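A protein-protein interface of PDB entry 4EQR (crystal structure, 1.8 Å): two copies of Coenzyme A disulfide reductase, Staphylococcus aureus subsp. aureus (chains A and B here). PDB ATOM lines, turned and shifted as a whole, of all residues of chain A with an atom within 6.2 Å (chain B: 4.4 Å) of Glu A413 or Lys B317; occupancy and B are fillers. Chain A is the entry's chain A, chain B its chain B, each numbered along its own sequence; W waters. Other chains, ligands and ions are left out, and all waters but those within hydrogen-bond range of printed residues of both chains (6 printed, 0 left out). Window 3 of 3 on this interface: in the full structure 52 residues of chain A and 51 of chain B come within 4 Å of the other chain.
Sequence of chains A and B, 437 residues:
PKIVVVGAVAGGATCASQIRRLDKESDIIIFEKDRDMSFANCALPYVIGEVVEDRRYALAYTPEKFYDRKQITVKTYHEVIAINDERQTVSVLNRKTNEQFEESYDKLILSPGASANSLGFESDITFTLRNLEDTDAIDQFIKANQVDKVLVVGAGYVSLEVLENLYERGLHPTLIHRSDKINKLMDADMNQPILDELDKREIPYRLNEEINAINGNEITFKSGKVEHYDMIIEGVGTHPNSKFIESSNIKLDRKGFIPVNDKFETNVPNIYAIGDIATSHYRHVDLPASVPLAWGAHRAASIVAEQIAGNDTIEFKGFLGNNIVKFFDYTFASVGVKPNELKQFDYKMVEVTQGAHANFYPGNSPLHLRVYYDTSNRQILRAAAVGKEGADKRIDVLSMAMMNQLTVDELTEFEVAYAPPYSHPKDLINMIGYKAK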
ATOM      1  N   ASP A 409     -12.310 -22.545 -33.473  1.00  0.00           N
ATOM      2  CA  ASP A 409     -11.114 -21.853 -33.017  1.00  0.00           C
ATOM      3  C   ASP A 409     -11.437 -20.538 -32.316  1.00  0.00           C
ATOM      4  O   ASP A 409     -10.733 -20.139 -31.387  1.00  0.00           O
ATOM      5  CB  ASP A 409     -10.181 -21.626 -34.197  1.00  0.00           C
ATOM      6  CG  ASP A 409      -9.893 -22.909 -34.934  1.00  0.00           C
ATOM      7  OD1 ASP A 409      -9.067 -23.705 -34.436  1.00  0.00           O
ATOM      8  OD2 ASP A 409     -10.515 -23.136 -35.990  1.00  0.00           O
ATOM      9  N   GLU A 410     -12.497 -19.870 -32.758  1.00  0.00           N
ATOM     10  CA  GLU A 410     -12.867 -18.569 -32.192  1.00  0.00           C
ATOM     11  C   GLU A 410     -13.433 -18.663 -30.776  1.00  0.00           C
ATOM     12  O   GLU A 410     -13.595 -17.646 -30.090  1.00  0.00           O
ATOM     13  CB  GLU A 410     -13.849 -17.834 -33.107  1.00  0.00           C
ATOM     14  CG  GLU A 410     -13.209 -17.306 -34.398  1.00  0.00           C
ATOM     15  CD  GLU A 410     -14.254 -16.802 -35.373  1.00  0.00           C
ATOM     16  OE1 GLU A 410     -14.967 -17.634 -35.966  1.00  0.00           O
ATOM     17  OE2 GLU A 410     -14.378 -15.574 -35.532  1.00  0.00           O
ATOM     18  N   LEU A 411     -13.727 -19.880 -30.336  1.00  0.00           N
ATOM     19  CA  LEU A 411     -14.236 -20.078 -28.986  1.00  0.00           C
ATOM     20  C   LEU A 411     -13.223 -19.615 -27.929  1.00  0.00           C
ATOM     21  O   LEU A 411     -13.594 -19.319 -26.784  1.00  0.00           O
ATOM     22  CB  LEU A 411     -14.636 -21.538 -28.758  1.00  0.00           C
ATOM     23  CG  LEU A 411     -15.821 -22.029 -29.593  1.00  0.00           C
ATOM     24  CD1 LEU A 411     -16.111 -23.494 -29.289  1.00  0.00           C
ATOM     25  CD2 LEU A 411     -17.037 -21.159 -29.319  1.00  0.00           C
ATOM     26  N   THR A 412     -11.946 -19.550 -28.300  1.00  0.00           N
ATOM     27  CA  THR A 412     -10.932 -19.054 -27.366  1.00  0.00           C
ATOM     28  C   THR A 412     -11.184 -17.595 -27.009  1.00  0.00           C
ATOM     29  O   THR A 412     -10.745 -17.119 -25.961  1.00  0.00           O
ATOM     30  CB  THR A 412      -9.494 -19.160 -27.943  1.00  0.00           C
ATOM     31  OG1 THR A 412      -9.409 -18.391 -29.150  1.00  0.00           O
ATOM     32  CG2 THR A 412      -9.149 -20.607 -28.246  1.00  0.00           C
ATOM     33  N   GLU A 413     -11.902 -16.895 -27.882  1.00  0.00           N
ATOM     34  CA  GLU A 413     -12.152 -15.464 -27.730  1.00  0.00           C
ATOM     35  C   GLU A 413     -13.419 -15.126 -26.961  1.00  0.00           C
ATOM     36  O   GLU A 413     -13.681 -13.955 -26.678  1.00  0.00           O
ATOM     37  CB  GLU A 413     -12.254 -14.816 -29.106  1.00  0.00           C
ATOM     38  CG  GLU A 413     -11.022 -15.021 -29.969  1.00  0.00           C
ATOM     39  CD  GLU A 413     -11.256 -14.586 -31.396  1.00  0.00           C
ATOM     40  OE1 GLU A 413     -12.255 -13.886 -31.642  1.00  0.00           O
ATOM     41  OE2 GLU A 413     -10.444 -14.951 -32.266  1.00  0.00           O
ATOM     42  N   PHE A 414     -14.222 -16.141 -26.663  1.00  0.00           N
ATOM     43  CA  PHE A 414     -15.463 -15.942 -25.927  1.00  0.00           C
ATOM     44  C   PHE A 414     -15.175 -15.365 -24.548  1.00  0.00           C
ATOM     45  O   PHE A 414     -14.389 -15.925 -23.797  1.00  0.00           O
ATOM     46  CB  PHE A 414     -16.213 -17.270 -25.791  1.00  0.00           C
ATOM     47  CG  PHE A 414     -17.319 -17.246 -24.770  1.00  0.00           C
ATOM     48  CD1 PHE A 414     -18.377 -16.360 -24.895  1.00  0.00           C
ATOM     49  CD2 PHE A 414     -17.307 -18.129 -23.696  1.00  0.00           C
ATOM     50  CE1 PHE A 414     -19.412 -16.353 -23.973  1.00  0.00           C
ATOM     51  CE2 PHE A 414     -18.337 -18.126 -22.756  1.00  0.00           C
ATOM     52  CZ  PHE A 414     -19.381 -17.234 -22.889  1.00  0.00           C
ATOM     53  N   GLU A 415     -15.804 -14.241 -24.223  1.00  0.00           N
ATOM     54  CA  GLU A 415     -15.547 -13.580 -22.954  1.00  0.00           C
ATOM     55  C   GLU A 415     -16.650 -13.943 -21.958  1.00  0.00           C
ATOM     56  O   GLU A 415     -17.723 -13.348 -21.957  1.00  0.00           O
ATOM     57  CB  GLU A 415     -15.442 -12.056 -23.141  1.00  0.00           C
ATOM     58  CG  GLU A 415     -14.957 -11.315 -21.894  1.00  0.00           C
ATOM     59  CD  GLU A 415     -14.694  -9.837 -22.129  1.00  0.00           C
ATOM     60  OE1 GLU A 415     -14.948  -9.043 -21.197  1.00  0.00           O
ATOM     61  OE2 GLU A 415     -14.250  -9.460 -23.237  1.00  0.00           O
ATOM     62  N   ASN A 430     -14.052 -21.777 -23.713  1.00  0.00           N
ATOM     63  CA  ASN A 430     -12.717 -21.381 -24.149  1.00  0.00           C
ATOM     64  C   ASN A 430     -11.822 -22.601 -24.346  1.00  0.00           C
ATOM     65  O   ASN A 430     -11.097 -22.673 -25.325  1.00  0.00           O
ATOM     66  CB  ASN A 430     -12.060 -20.422 -23.147  1.00  0.00           C
ATOM     67  CG  ASN A 430     -12.865 -19.150 -22.933  1.00  0.00           C
ATOM     68  OD1 ASN A 430     -13.116 -18.751 -21.792  1.00  0.00           O
ATOM     69  ND2 ASN A 430     -13.251 -18.495 -24.025  1.00  0.00           N
ATOM     70  N   TYR A 434      -9.153 -23.847 -27.214  1.00  0.00           N
ATOM     71  CA  TYR A 434      -7.725 -24.090 -27.009  1.00  0.00           C
ATOM     72  C   TYR A 434      -7.349 -25.516 -27.379  1.00  0.00           C
ATOM     73  O   TYR A 434      -6.236 -25.776 -27.835  1.00  0.00           O
ATOM     74  CB  TYR A 434      -7.302 -23.788 -25.565  1.00  0.00           C
ATOM     75  CG  TYR A 434      -7.318 -22.321 -25.208  1.00  0.00           C
ATOM     76  CD1 TYR A 434      -8.162 -21.838 -24.218  1.00  0.00           C
ATOM     77  CD2 TYR A 434      -6.488 -21.410 -25.871  1.00  0.00           C
ATOM     78  CE1 TYR A 434      -8.182 -20.497 -23.889  1.00  0.00           C
ATOM     79  CE2 TYR A 434      -6.505 -20.058 -25.550  1.00  0.00           C
ATOM     80  CZ  TYR A 434      -7.351 -19.608 -24.554  1.00  0.00           C
ATOM     81  OH  TYR A 434      -7.383 -18.266 -24.214  1.00  0.00           O
ATOM     82  N   HIS B 281      -8.805  -1.794 -25.826  1.00  0.00           N
ATOM     83  CA  HIS B 281      -9.976  -1.162 -26.415  1.00  0.00           C
ATOM     84  C   HIS B 281     -11.115  -2.160 -26.367  1.00  0.00           C
ATOM     85  O   HIS B 281     -10.884  -3.348 -26.175  1.00  0.00           O
ATOM     86  CB  HIS B 281      -9.696  -0.788 -27.868  1.00  0.00           C
ATOM     87  CG  HIS B 281      -9.225  -1.943 -28.694  1.00  0.00           C
ATOM     88  ND1 HIS B 281     -10.087  -2.765 -29.387  1.00  0.00           N
ATOM     89  CD2 HIS B 281      -7.981  -2.434 -28.911  1.00  0.00           C
ATOM     90  CE1 HIS B 281      -9.395  -3.699 -30.013  1.00  0.00           C
ATOM     91  NE2 HIS B 281      -8.115  -3.524 -29.737  1.00  0.00           N
ATOM     92  N   ARG B 283     -14.069  -4.449 -28.046  1.00  0.00           N
ATOM     93  CA  ARG B 283     -14.151  -5.239 -29.259  1.00  0.00           C
ATOM     94  C   ARG B 283     -15.267  -4.737 -30.177  1.00  0.00           C
ATOM     95  O   ARG B 283     -15.153  -4.789 -31.401  1.00  0.00           O
ATOM     96  CB  ARG B 283     -14.374  -6.714 -28.907  1.00  0.00           C
ATOM     97  CG  ARG B 283     -14.768  -7.552 -30.106  1.00  0.00           C
ATOM     98  CD  ARG B 283     -14.607  -9.046 -29.880  1.00  0.00           C
ATOM     99  NE  ARG B 283     -14.855  -9.767 -31.128  1.00  0.00           N
ATOM    100  CZ  ARG B 283     -14.379 -10.977 -31.420  1.00  0.00           C
ATOM    101  NH1 ARG B 283     -13.609 -11.630 -30.559  1.00  0.00           N
ATOM    102  NH2 ARG B 283     -14.675 -11.537 -32.589  1.00  0.00           N
ATOM    103  N   TRP B 295     -10.667 -12.990 -16.528  1.00  0.00           N
ATOM    104  CA  TRP B 295     -10.737 -13.453 -17.916  1.00  0.00           C
ATOM    105  C   TRP B 295      -9.657 -12.796 -18.756  1.00  0.00           C
ATOM    106  O   TRP B 295      -8.975 -13.458 -19.542  1.00  0.00           O
ATOM    107  CB  TRP B 295     -12.097 -13.164 -18.563  1.00  0.00           C
ATOM    108  CG  TRP B 295     -12.153 -13.696 -19.962  1.00  0.00           C
ATOM    109  CD1 TRP B 295     -12.486 -14.965 -20.344  1.00  0.00           C
ATOM    110  CD2 TRP B 295     -11.840 -12.984 -21.163  1.00  0.00           C
ATOM    111  NE1 TRP B 295     -12.411 -15.081 -21.710  1.00  0.00           N
ATOM    112  CE2 TRP B 295     -12.019 -13.878 -22.239  1.00  0.00           C
ATOM    113  CE3 TRP B 295     -11.459 -11.668 -21.441  1.00  0.00           C
ATOM    114  CZ2 TRP B 295     -11.808 -13.507 -23.567  1.00  0.00           C
ATOM    115  CZ3 TRP B 295     -11.244 -11.300 -22.759  1.00  0.00           C
ATOM    116  CH2 TRP B 295     -11.417 -12.216 -23.804  1.00  0.00           C
ATOM    117  N   ARG B 299      -6.659 -14.451 -20.780  1.00  0.00           N
ATOM    118  CA  ARG B 299      -6.672 -14.395 -22.238  1.00  0.00           C
ATOM    119  C   ARG B 299      -5.378 -13.758 -22.747  1.00  0.00           C
ATOM    120  O   ARG B 299      -4.761 -14.245 -23.699  1.00  0.00           O
ATOM    121  CB  ARG B 299      -7.879 -13.612 -22.751  1.00  0.00           C
ATOM    122  CG  ARG B 299      -7.896 -13.448 -24.278  1.00  0.00           C
ATOM    123  CD  ARG B 299      -8.022 -14.824 -24.974  1.00  0.00           C
ATOM    124  NE  ARG B 299      -7.858 -14.716 -26.419  1.00  0.00           N
ATOM    125  CZ  ARG B 299      -7.295 -15.642 -27.195  1.00  0.00           C
ATOM    126  NH1 ARG B 299      -7.179 -15.438 -28.505  1.00  0.00           N
ATOM    127  NH2 ARG B 299      -6.843 -16.769 -26.672  1.00  0.00           N
ATOM    128  N   GLU B 315      -3.891 -12.410 -32.263  1.00  0.00           N
ATOM    129  CA  GLU B 315      -3.946 -11.101 -31.613  1.00  0.00           C
ATOM    130  C   GLU B 315      -5.267 -10.880 -30.890  1.00  0.00           C
ATOM    131  O   GLU B 315      -6.285 -11.489 -31.220  1.00  0.00           O
ATOM    132  CB  GLU B 315      -3.723  -9.966 -32.623  1.00  0.00           C
ATOM    133  CG  GLU B 315      -2.362 -10.011 -33.310  1.00  0.00           C
ATOM    134  CD  GLU B 315      -2.060  -8.764 -34.120  1.00  0.00           C
ATOM    135  OE1 GLU B 315      -2.718  -7.724 -33.909  1.00  0.00           O
ATOM    136  OE2 GLU B 315      -1.145  -8.826 -34.967  1.00  0.00           O
ATOM    137  N   PHE B 316      -5.236  -9.989 -29.905  1.00  0.00           N
ATOM    138  CA  PHE B 316      -6.412  -9.638 -29.122  1.00  0.00           C
ATOM    139  C   PHE B 316      -7.401  -8.937 -30.030  1.00  0.00           C
ATOM    140  O   PHE B 316      -6.995  -8.198 -30.926  1.00  0.00           O
ATOM    141  CB  PHE B 316      -5.994  -8.680 -28.000  1.00  0.00           C
ATOM    142  CG  PHE B 316      -7.027  -8.495 -26.925  1.00  0.00           C
ATOM    143  CD1 PHE B 316      -7.677  -9.589 -26.364  1.00  0.00           C
ATOM    144  CD2 PHE B 316      -7.327  -7.226 -26.455  1.00  0.00           C
ATOM    145  CE1 PHE B 316      -8.601  -9.416 -25.356  1.00  0.00           C
ATOM    146  CE2 PHE B 316      -8.262  -7.044 -25.447  1.00  0.00           C
ATOM    147  CZ  PHE B 316      -8.899  -8.139 -24.901  1.00  0.00           C
ATOM    148  N   LYS B 317      -8.695  -9.157 -29.807  1.00  0.00           N
ATOM    149  CA  LYS B 317      -9.695  -8.424 -30.574  1.00  0.00           C
ATOM    150  C   LYS B 317     -10.451  -7.379 -29.744  1.00  0.00           C
ATOM    151  O   LYS B 317     -11.415  -6.773 -30.214  1.00  0.00           O
ATOM    152  CB  LYS B 317     -10.636  -9.396 -31.304  1.00  0.00           C
ATOM    153  CG  LYS B 317      -9.906 -10.127 -32.441  1.00  0.00           C
ATOM    154  CD  LYS B 317     -10.697 -11.271 -33.028  1.00  0.00           C
ATOM    155  CE  LYS B 317      -9.914 -11.884 -34.183  1.00  0.00           C
ATOM    156  NZ  LYS B 317     -10.327 -13.281 -34.471  1.00  0.00           N
ATOM    157  N   GLY B 318      -9.999  -7.155 -28.514  1.00  0.00           N
ATOM    158  CA  GLY B 318     -10.605  -6.144 -27.665  1.00  0.00           C
ATOM    159  C   GLY B 318     -11.488  -6.753 -26.585  1.00  0.00           C
ATOM    160  O   GLY B 318     -11.810  -7.946 -26.621  1.00  0.00           O
ATOM    161  N   MET B 403     -19.867 -10.347 -29.586  1.00  0.00           N
ATOM    162  CA  MET B 403     -18.677 -10.839 -30.268  1.00  0.00           C
ATOM    163  C   MET B 403     -18.941 -10.971 -31.769  1.00  0.00           C
ATOM    164  O   MET B 403     -18.043 -10.812 -32.592  1.00  0.00           O
ATOM    165  CB  MET B 403     -18.320 -12.221 -29.723  1.00  0.00           C
ATOM    166  CG  MET B 403     -16.848 -12.551 -29.723  1.00  0.00           C
ATOM    167  SD  MET B 403     -16.573 -14.276 -29.275  1.00  0.00           S
ATOM    168  CE  MET B 403     -16.340 -14.983 -30.899  1.00  0.00           C
HETATM  169  O   HOH W   1     -13.392 -13.611 -34.035  1.00  0.00           O
HETATM  170  O   HOH W   2     -17.655 -13.155 -25.948  1.00  0.00           O
HETATM  171  O   HOH W   3      -6.867 -17.826 -30.306  1.00  0.00           O
HETATM  172  O   HOH W   4     -15.318 -11.719 -27.322  1.00  0.00           O
HETATM  173  O   HOH W   5     -12.913 -11.560 -27.769  1.00  0.00           O
HETATM  174  O   HOH W   6     -13.749  -9.884 -26.002  1.00  0.00           O
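The side-chain carboxylate (OE1) of Glu A413 lies within salt-bridge range of the guanidinium group (NH1) of Arg B283, at 2.8 Å. The side-chain amino group (NZ) of Lys B317 is in salt-bridge range of the side-chain carboxylate (OE2) of Glu A413 (2.8 Å). The indole nitrogen of Trp B295 sits at hydrogen-bond distance from the backbone carbonyl oxygen of Phe A414, 3.0 Å away. OH of Tyr A434 sits at hydrogen-bond distance from NH2 of Arg B299, at 2.9 Å.
The backbone carbonyl oxygen (O) of Asp A409 sits at hydrogen-bond distance from the side-chain hydroxyl (OG1) of Thr A412. The backbone carbonyl oxygen (O) of Leu A411 is in hydrogen-bond range of the side-chain amide nitrogen (ND2) of Asn A430, 2.9 Å away. The backbone carbonyl oxygen (O) of Thr A412 is in hydrogen-bond range of the side-chain amide nitrogen (ND2) of Asn A430, 3.5 Å away. O of Phe A414 sits at hydrogen-bond distance from ND2 of Asn A430 (2.8 Å). NH2 of Arg B283 sits at hydrogen-bond distance from O of Met B403 (3.4 Å).
CE of Met B403 touches O of Glu A410, at 3.9 Å. Arg B299 touches Thr A412. Glu A413 touches Trp B295. Glu A413 touches Met B403. Phe A414 touches Met B403 (CA to SD, 3.9 Å). Glu A415 touches Trp B295. NE1 of Trp B295 touches OD1 of Asn A430, at 3.7 Å.
Glu A413 touches just these residues of chain B: Arg B283, Trp B295, Lys B317 and Met B403. Printed residues of chain A within 4 Å of Lys B317: Glu A413. Of the printed residues of chain B, Thr A412 touches Arg B299. Of the printed residues of chain B, Tyr A434 touches Arg B299. Glu B315 touches none of the printed residues of chain A. Phe B316 touches none of the printed residues of chain A. The nearest residue of chain A that does not touch Lys B317 is Glu A410 (4.8 Å).
Of the 9 printed residues of chain B, 5 touch a printed residue of chain A. Hydrophobic or aromatic side chains of chain B that line the printed part of chain A: Trp B295 and Met B403. Hydrophobic or aromatic side chains of chain A that line the printed part of chain B: Tyr A434. Along chain A the printed residues that touch a printed residue of chain B span positions 410 to 434. Among the printed residues, Asp or Glu carboxylates within 4 Å of a Lys or Arg side-chain nitrogen of the other chain: Glu A413 with Arg B283 and Glu A413 with Lys B317.
No position is printed for both chains.
Water W1 lies within hydrogen-bond range of the side-chain carboxylate of Glu A410 (2.7 Å), the side-chain carboxylate of Glu A413 (2.7 Å), the guanidinium group of Arg B283 (2.8 Å) and the side-chain amino group of Lys B317 (3.1 Å). Water W5 lies within hydrogen-bond range of the backbone carbonyl oxygen (O) of Glu A413 (2.7 Å) and the guanidinium group (NH1) of Arg B283 (2.9 Å). Water W2 lies within hydrogen-bond range of N of Glu A415 and SD of Met B403. Water W6 lies within hydrogen-bond range of the backbone carbonyl oxygen (O) of Gly B318 (2.8 Å) and the side-chain carboxylate (OE2) of Glu A415 (2.8 Å). Water W4 lies within hydrogen-bond range of O of Glu A413 (2.8 Å) and SD of Met B403 (3.5 Å). Water W3 bridges OG1 of Thr A412 (2.8 Å) and NH1 of Arg B299 (3.0 Å).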
